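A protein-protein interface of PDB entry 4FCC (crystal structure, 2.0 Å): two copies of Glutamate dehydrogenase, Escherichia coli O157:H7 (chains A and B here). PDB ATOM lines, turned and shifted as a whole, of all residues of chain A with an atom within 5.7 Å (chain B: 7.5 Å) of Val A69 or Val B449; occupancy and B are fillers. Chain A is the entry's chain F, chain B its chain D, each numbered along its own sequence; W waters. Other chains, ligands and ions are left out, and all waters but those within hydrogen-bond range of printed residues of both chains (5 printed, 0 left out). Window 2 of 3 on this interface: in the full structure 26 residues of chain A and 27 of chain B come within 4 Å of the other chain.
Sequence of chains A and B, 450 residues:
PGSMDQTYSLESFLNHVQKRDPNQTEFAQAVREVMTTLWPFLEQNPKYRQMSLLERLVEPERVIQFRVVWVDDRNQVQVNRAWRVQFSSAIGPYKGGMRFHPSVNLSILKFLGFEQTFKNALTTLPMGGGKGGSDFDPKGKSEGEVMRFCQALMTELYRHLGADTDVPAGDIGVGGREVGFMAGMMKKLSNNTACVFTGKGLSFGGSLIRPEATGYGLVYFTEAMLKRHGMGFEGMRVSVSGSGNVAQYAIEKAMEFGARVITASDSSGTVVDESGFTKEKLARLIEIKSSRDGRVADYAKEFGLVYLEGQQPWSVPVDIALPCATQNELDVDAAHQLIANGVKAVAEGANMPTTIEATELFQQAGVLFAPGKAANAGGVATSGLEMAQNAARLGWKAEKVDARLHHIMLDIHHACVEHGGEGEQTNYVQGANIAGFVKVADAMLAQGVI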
ATOM      1  N   ARG A  67      11.750 -20.894 -20.014  1.00  0.00           N
ATOM      2  CA  ARG A  67      12.668 -20.441 -21.044  1.00  0.00           C
ATOM      3  C   ARG A  67      13.932 -19.869 -20.406  1.00  0.00           C
ATOM      4  O   ARG A  67      13.863 -19.190 -19.381  1.00  0.00           O
ATOM      5  CB  ARG A  67      11.977 -19.371 -21.894  1.00  0.00           C
ATOM      6  CG  ARG A  67      12.774 -18.838 -23.059  1.00  0.00           C
ATOM      7  CD  ARG A  67      11.991 -17.790 -23.808  1.00  0.00           C
ATOM      8  NE  ARG A  67      11.863 -16.535 -23.066  1.00  0.00           N
ATOM      9  CZ  ARG A  67      11.099 -15.512 -23.452  1.00  0.00           C
ATOM     10  NH1 ARG A  67      10.376 -15.583 -24.572  1.00  0.00           N
ATOM     11  NH2 ARG A  67      11.058 -14.411 -22.716  1.00  0.00           N
ATOM     12  N   VAL A  68      15.080 -20.140 -21.020  1.00  0.00           N
ATOM     13  CA  VAL A  68      16.328 -19.502 -20.622  1.00  0.00           C
ATOM     14  C   VAL A  68      16.979 -18.817 -21.816  1.00  0.00           C
ATOM     15  O   VAL A  68      17.373 -19.483 -22.798  1.00  0.00           O
ATOM     16  CB  VAL A  68      17.318 -20.515 -19.973  1.00  0.00           C
ATOM     17  CG1 VAL A  68      18.617 -19.819 -19.585  1.00  0.00           C
ATOM     18  CG2 VAL A  68      16.688 -21.167 -18.738  1.00  0.00           C
ATOM     19  N   VAL A  69      17.085 -17.489 -21.755  1.00  0.00           N
ATOM     20  CA  VAL A  69      17.716 -16.748 -22.852  1.00  0.00           C
ATOM     21  C   VAL A  69      19.073 -16.166 -22.456  1.00  0.00           C
ATOM     22  O   VAL A  69      19.186 -15.493 -21.433  1.00  0.00           O
ATOM     23  CB  VAL A  69      16.829 -15.627 -23.439  1.00  0.00           C
ATOM     24  CG1 VAL A  69      17.359 -15.237 -24.834  1.00  0.00           C
ATOM     25  CG2 VAL A  69      15.369 -16.072 -23.543  1.00  0.00           C
ATOM     26  N   TRP A  70      20.091 -16.418 -23.285  1.00  0.00           N
ATOM     27  CA  TRP A  70      21.455 -15.988 -23.004  1.00  0.00           C
ATOM     28  C   TRP A  70      22.251 -15.740 -24.292  1.00  0.00           C
ATOM     29  O   TRP A  70      21.857 -16.164 -25.372  1.00  0.00           O
ATOM     30  CB  TRP A  70      22.173 -17.023 -22.121  1.00  0.00           C
ATOM     31  CG  TRP A  70      22.351 -18.345 -22.791  1.00  0.00           C
ATOM     32  CD1 TRP A  70      21.400 -19.313 -22.977  1.00  0.00           C
ATOM     33  CD2 TRP A  70      23.552 -18.842 -23.389  1.00  0.00           C
ATOM     34  NE1 TRP A  70      21.939 -20.377 -23.663  1.00  0.00           N
ATOM     35  CE2 TRP A  70      23.257 -20.111 -23.926  1.00  0.00           C
ATOM     36  CE3 TRP A  70      24.848 -18.332 -23.532  1.00  0.00           C
ATOM     37  CZ2 TRP A  70      24.218 -20.881 -24.593  1.00  0.00           C
ATOM     38  CZ3 TRP A  70      25.796 -19.097 -24.195  1.00  0.00           C
ATOM     39  CH2 TRP A  70      25.477 -20.354 -24.713  1.00  0.00           C
ATOM     40  N   VAL A  71      23.381 -15.054 -24.158  1.00  0.00           N
ATOM     41  CA  VAL A  71      24.184 -14.663 -25.309  1.00  0.00           C
ATOM     42  C   VAL A  71      25.511 -15.430 -25.352  1.00  0.00           C
ATOM     43  O   VAL A  71      26.242 -15.462 -24.370  1.00  0.00           O
ATOM     44  CB  VAL A  71      24.452 -13.150 -25.281  1.00  0.00           C
ATOM     45  CG1 VAL A  71      25.113 -12.710 -26.557  1.00  0.00           C
ATOM     46  CG2 VAL A  71      23.129 -12.365 -25.061  1.00  0.00           C
ATOM     47  N   VAL A  77      22.228 -14.637 -29.787  1.00  0.00           N
ATOM     48  CA  VAL A  77      21.252 -14.954 -28.751  1.00  0.00           C
ATOM     49  C   VAL A  77      20.841 -16.422 -28.871  1.00  0.00           C
ATOM     50  O   VAL A  77      20.527 -16.898 -29.961  1.00  0.00           O
ATOM     51  CB  VAL A  77      20.018 -14.031 -28.823  1.00  0.00           C
ATOM     52  CG1 VAL A  77      18.887 -14.570 -27.946  1.00  0.00           C
ATOM     53  CG2 VAL A  77      20.394 -12.587 -28.428  1.00  0.00           C
ATOM     54  N   GLN A  78      20.880 -17.140 -27.754  1.00  0.00           N
ATOM     55  CA  GLN A  78      20.516 -18.551 -27.729  1.00  0.00           C
ATOM     56  C   GLN A  78      19.325 -18.778 -26.802  1.00  0.00           C
ATOM     57  O   GLN A  78      19.170 -18.081 -25.800  1.00  0.00           O
ATOM     58  CB  GLN A  78      21.693 -19.398 -27.249  1.00  0.00           C
ATOM     59  CG  GLN A  78      22.971 -19.242 -28.081  1.00  0.00           C
ATOM     60  CD  GLN A  78      22.809 -19.722 -29.518  1.00  0.00           C
ATOM     61  OE1 GLN A  78      21.922 -20.521 -29.824  1.00  0.00           O
ATOM     62  NE2 GLN A  78      23.660 -19.221 -30.407  1.00  0.00           N
ATOM     63  N   VAL A  79      18.490 -19.756 -27.138  1.00  0.00           N
ATOM     64  CA  VAL A  79      17.334 -20.077 -26.326  1.00  0.00           C
ATOM     65  C   VAL A  79      17.379 -21.533 -25.879  1.00  0.00           C
ATOM     66  O   VAL A  79      17.452 -22.436 -26.708  1.00  0.00           O
ATOM     67  CB  VAL A  79      16.023 -19.829 -27.086  1.00  0.00           C
ATOM     68  CG1 VAL A  79      14.835 -20.146 -26.187  1.00  0.00           C
ATOM     69  CG2 VAL A  79      15.948 -18.394 -27.557  1.00  0.00           C
ATOM     70  N   ASN A  80      17.330 -21.762 -24.569  1.00  0.00           N
ATOM     71  CA  ASN A  80      17.275 -23.126 -24.056  1.00  0.00           C
ATOM     72  C   ASN A  80      16.086 -23.343 -23.137  1.00  0.00           C
ATOM     73  O   ASN A  80      15.509 -22.392 -22.612  1.00  0.00           O
ATOM     74  CB  ASN A  80      18.578 -23.507 -23.338  1.00  0.00           C
ATOM     75  CG  ASN A  80      19.723 -23.773 -24.312  1.00  0.00           C
ATOM     76  OD1 ASN A  80      20.517 -22.883 -24.589  1.00  0.00           O
ATOM     77  ND2 ASN A  80      19.791 -24.993 -24.850  1.00  0.00           N
ATOM     78  N   ALA A 152      21.442 -16.521 -16.196  1.00  0.00           N
ATOM     79  CA  ALA A 152      20.173 -16.384 -16.899  1.00  0.00           C
ATOM     80  C   ALA A 152      19.149 -17.361 -16.327  1.00  0.00           C
ATOM     81  O   ALA A 152      18.001 -17.000 -16.061  1.00  0.00           O
ATOM     82  CB  ALA A 152      20.362 -16.636 -18.405  1.00  0.00           C
ATOM     83  N   MET B  51      18.107 -11.090 -32.638  1.00  0.00           N
ATOM     84  CA  MET B  51      17.975 -11.432 -31.222  1.00  0.00           C
ATOM     85  C   MET B  51      17.251 -12.766 -31.038  1.00  0.00           C
ATOM     86  O   MET B  51      16.502 -12.933 -30.074  1.00  0.00           O
ATOM     87  CB  MET B  51      17.239 -10.330 -30.443  1.00  0.00           C
ATOM     88  CG  MET B  51      17.585  -8.888 -30.809  1.00  0.00           C
ATOM     89  SD  MET B  51      19.200  -8.327 -30.258  1.00  0.00           S
ATOM     90  CE  MET B  51      18.703  -7.088 -29.067  1.00  0.00           C
ATOM     91  N   SER B  52      17.507 -13.707 -31.950  1.00  0.00           N
ATOM     92  CA  SER B  52      16.783 -14.985 -32.029  1.00  0.00           C
ATOM     93  C   SER B  52      15.312 -14.874 -31.587  1.00  0.00           C
ATOM     94  O   SER B  52      14.855 -15.518 -30.638  1.00  0.00           O
ATOM     95  CB  SER B  52      17.518 -16.078 -31.269  1.00  0.00           C
ATOM     96  OG  SER B  52      16.760 -17.271 -31.285  1.00  0.00           O
ATOM     97  N   GLU B  55      12.603 -18.084 -32.007  1.00  0.00           N
ATOM     98  CA  GLU B  55      12.890 -19.043 -30.950  1.00  0.00           C
ATOM     99  C   GLU B  55      12.422 -18.557 -29.583  1.00  0.00           C
ATOM    100  O   GLU B  55      11.862 -19.331 -28.800  1.00  0.00           O
ATOM    101  CB  GLU B  55      14.385 -19.313 -30.866  1.00  0.00           C
ATOM    102  CG  GLU B  55      14.903 -20.387 -31.801  1.00  0.00           C
ATOM    103  CD  GLU B  55      16.249 -20.895 -31.339  1.00  0.00           C
ATOM    104  OE1 GLU B  55      17.232 -20.131 -31.437  1.00  0.00           O
ATOM    105  OE2 GLU B  55      16.317 -22.040 -30.842  1.00  0.00           O
ATOM    106  N   ARG B  56      12.681 -17.288 -29.282  1.00  0.00           N
ATOM    107  CA  ARG B  56      12.211 -16.726 -28.020  1.00  0.00           C
ATOM    108  C   ARG B  56      10.690 -16.730 -27.987  1.00  0.00           C
ATOM    109  O   ARG B  56      10.089 -17.033 -26.958  1.00  0.00           O
ATOM    110  CB  ARG B  56      12.721 -15.303 -27.816  1.00  0.00           C
ATOM    111  CG  ARG B  56      14.214 -15.200 -27.555  1.00  0.00           C
ATOM    112  CD  ARG B  56      14.505 -13.928 -26.812  1.00  0.00           C
ATOM    113  NE  ARG B  56      14.933 -12.845 -27.678  1.00  0.00           N
ATOM    114  CZ  ARG B  56      14.870 -11.559 -27.352  1.00  0.00           C
ATOM    115  NH1 ARG B  56      14.367 -11.172 -26.183  1.00  0.00           N
ATOM    116  NH2 ARG B  56      15.296 -10.651 -28.209  1.00  0.00           N
ATOM    117  N   GLU B  59       9.012 -20.328 -27.330  1.00  0.00           N
ATOM    118  CA  GLU B  59       9.303 -20.935 -26.039  1.00  0.00           C
ATOM    119  C   GLU B  59       8.631 -20.127 -24.935  1.00  0.00           C
ATOM    120  O   GLU B  59       9.018 -18.983 -24.673  1.00  0.00           O
ATOM    121  CB  GLU B  59      10.810 -21.010 -25.814  1.00  0.00           C
ATOM    122  CG  GLU B  59      11.238 -21.669 -24.497  1.00  0.00           C
ATOM    123  CD  GLU B  59      10.980 -23.168 -24.452  1.00  0.00           C
ATOM    124  OE1 GLU B  59      10.737 -23.778 -25.517  1.00  0.00           O
ATOM    125  OE2 GLU B  59      11.018 -23.740 -23.343  1.00  0.00           O
ATOM    126  N   MET B 444       9.159  -7.300 -27.152  1.00  0.00           N
ATOM    127  CA  MET B 444      10.256  -8.208 -26.836  1.00  0.00           C
ATOM    128  C   MET B 444      11.592  -7.579 -27.220  1.00  0.00           C
ATOM    129  O   MET B 444      12.555  -7.646 -26.470  1.00  0.00           O
ATOM    130  CB  MET B 444      10.102  -9.538 -27.598  1.00  0.00           C
ATOM    131  CG  MET B 444       8.824 -10.321 -27.309  1.00  0.00           C
ATOM    132  SD  MET B 444       8.641 -11.832 -28.319  1.00  0.00           S
ATOM    133  CE  MET B 444      10.064 -12.777 -27.771  1.00  0.00           C
ATOM    134  N   LEU B 445      11.656  -6.991 -28.409  1.00  0.00           N
ATOM    135  CA  LEU B 445      12.884  -6.333 -28.836  1.00  0.00           C
ATOM    136  C   LEU B 445      13.291  -5.236 -27.842  1.00  0.00           C
ATOM    137  O   LEU B 445      14.460  -5.126 -27.471  1.00  0.00           O
ATOM    138  CB  LEU B 445      12.717  -5.736 -30.235  1.00  0.00           C
ATOM    139  CG  LEU B 445      12.495  -6.752 -31.361  1.00  0.00           C
ATOM    140  CD1 LEU B 445      12.460  -6.058 -32.711  1.00  0.00           C
ATOM    141  CD2 LEU B 445      13.546  -7.821 -31.320  1.00  0.00           C
ATOM    142  N   ALA B 446      12.316  -4.435 -27.416  1.00  0.00           N
ATOM    143  CA  ALA B 446      12.577  -3.283 -26.546  1.00  0.00           C
ATOM    144  C   ALA B 446      13.060  -3.649 -25.151  1.00  0.00           C
ATOM    145  O   ALA B 446      13.822  -2.902 -24.518  1.00  0.00           O
ATOM    146  CB  ALA B 446      11.325  -2.400 -26.448  1.00  0.00           C
ATOM    147  N   GLN B 447      12.604  -4.789 -24.654  1.00  0.00           N
ATOM    148  CA  GLN B 447      12.820  -5.116 -23.239  1.00  0.00           C
ATOM    149  C   GLN B 447      14.055  -5.984 -22.973  1.00  0.00           C
ATOM    150  O   GLN B 447      14.241  -6.517 -21.872  1.00  0.00           O
ATOM    151  CB  GLN B 447      11.544  -5.712 -22.639  1.00  0.00           C
ATOM    152  CG  GLN B 447      10.501  -4.629 -22.373  1.00  0.00           C
ATOM    153  CD  GLN B 447       9.115  -5.157 -22.036  1.00  0.00           C
ATOM    154  OE1 GLN B 447       8.703  -5.140 -20.876  1.00  0.00           O
ATOM    155  NE2 GLN B 447       8.375  -5.584 -23.055  1.00  0.00           N
ATOM    156  N   GLY B 448      14.900  -6.129 -23.987  1.00  0.00           N
ATOM    157  CA  GLY B 448      16.177  -6.790 -23.799  1.00  0.00           C
ATOM    158  C   GLY B 448      16.137  -8.309 -23.763  1.00  0.00           C
ATOM    159  O   GLY B 448      15.081  -8.924 -23.863  1.00  0.00           O
ATOM    160  N   VAL B 449      17.312  -8.909 -23.609  1.00  0.00           N
ATOM    161  CA  VAL B 449      17.444 -10.354 -23.585  1.00  0.00           C
ATOM    162  C   VAL B 449      17.146 -10.822 -22.170  1.00  0.00           C
ATOM    163  O   VAL B 449      17.990 -10.696 -21.285  1.00  0.00           O
ATOM    164  CB  VAL B 449      18.877 -10.768 -24.005  1.00  0.00           C
ATOM    165  CG1 VAL B 449      19.063 -12.273 -23.940  1.00  0.00           C
ATOM    166  CG2 VAL B 449      19.184 -10.258 -25.405  1.00  0.00           C
ATOM    167  N   ILE B 450      15.928 -11.312 -21.945  1.00  0.00           N
ATOM    168  CA  ILE B 450      15.524 -11.806 -20.620  1.00  0.00           C
ATOM    169  C   ILE B 450      14.890 -13.191 -20.735  1.00  0.00           C
ATOM    170  O   ILE B 450      14.307 -13.535 -21.776  1.00  0.00           O
ATOM    171  CB  ILE B 450      14.537 -10.841 -19.908  1.00  0.00           C
ATOM    172  CG1 ILE B 450      13.249 -10.669 -20.709  1.00  0.00           C
ATOM    173  CG2 ILE B 450      15.186  -9.485 -19.645  1.00  0.00           C
ATOM    174  CD1 ILE B 450      12.088 -11.529 -20.226  1.00  0.00           C
HETATM  175  O   HOH W   1      13.568 -12.803 -24.238  1.00  0.00           O
HETATM  176  O   HOH W   2       7.460 -16.674 -24.723  1.00  0.00           O
HETATM  177  O   HOH W   3      18.784 -21.203 -29.717  1.00  0.00           O
HETATM  178  O   HOH W   4       9.713 -23.115 -21.220  1.00  0.00           O
HETATM  179  O   HOH W   5      13.266 -15.892 -20.495  1.00  0.00           O
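NH1 of Arg A67 lies within hydrogen-bond range of O of Arg B56 (2.8 Å).
O of Ile B450 is in hydrogen-bond range of NH2 of Arg A67 (3.5 Å).
O of Glu B59 touches CD of Arg A67, 3.3 Å away.
Val A69 touches Arg B56.
CG1 of Val A69 touches CG1 of Val B449, at 3.5 Å.
Val A69 touches Ile B450 (CG2 to O, 3.3 Å).
Val A77 touches Met B51.
Val A77 touches Ser B52 (O to CB, 3.4 Å).
CG2 of Val A79 touches OG of Ser B52 (3.98 Å).
Glu B55 touches Val A79.
Val A79 touches Arg B56 (CG2 to CG, 3.6 Å).
Of the 12 printed residues of chain B, 7 touch a printed residue of chain A.
Hydrophobic or aromatic side chains of chain B that line the printed part of chain A: Val B449 and Ile B450.
Of the 10 printed residues of chain A, 4 touch a printed residue of chain B.
Among the printed residues, 11 pairs touch across the chains.
No position is printed for both chains.
Of the 11 pairs that touch across the chains among the printed residues, none has its exchanged pair printed and touching as well.
Of chain B, only Arg B56 (3.7 Å), Val B449 (3.5 Å) and Ile B450 (3.3 Å) come within 4 Å of Val A69.
Printed residues of chain A within 4 Å of Val B449: Val A69.
Of the printed residues of chain A, Glu B55 touches Val A79.
Of the printed residues of chain A, Met B51 touches Val A77.
Of the printed residues of chain A, Ile B450 touches Arg A67 (3.5 Å) and Val A69 (3.3 Å).
Val A68 touches none of the printed residues of chain B.
The guanidinium group of Arg B56 is in hydrogen-bond range of the backbone carbonyl oxygen of Met B51 (2.9 Å).
OG of Ser B52 is in hydrogen-bond range of OE1 of Glu B55, 2.9 Å away.
The backbone carbonyl oxygen (O) of Gly B448 sits at hydrogen-bond distance from the guanidinium group (NH1) of Arg B56.
Water W3 lies within hydrogen-bond range of OE1 of Glu B55 (2.6 Å), N of Val A79 (3.0 Å) and OE1 of Gln A78 (3.2 Å).
Water W4 lies within hydrogen-bond range of the side-chain carboxylate (OE2) of Glu B59 (2.6 Å) and the backbone NH (N) of Arg A67 (3.2 Å).
Water W1 lies within hydrogen-bond range of NH1 of Arg B56 (2.7 Å), O of Ile B450 (2.7 Å) and NH2 of Arg A67 (3.3 Å).
Water W2 lies within hydrogen-bond range of the backbone carbonyl oxygen of Glu B59 (2.8 Å), the guanidinium group of Arg A67 (3.1 Å) and the backbone carbonyl oxygen of Arg B56 (3.5 Å).
Water W5 bridges O of Ile B450 (2.9 Å) and NE of Arg A67 (3.0 Å).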
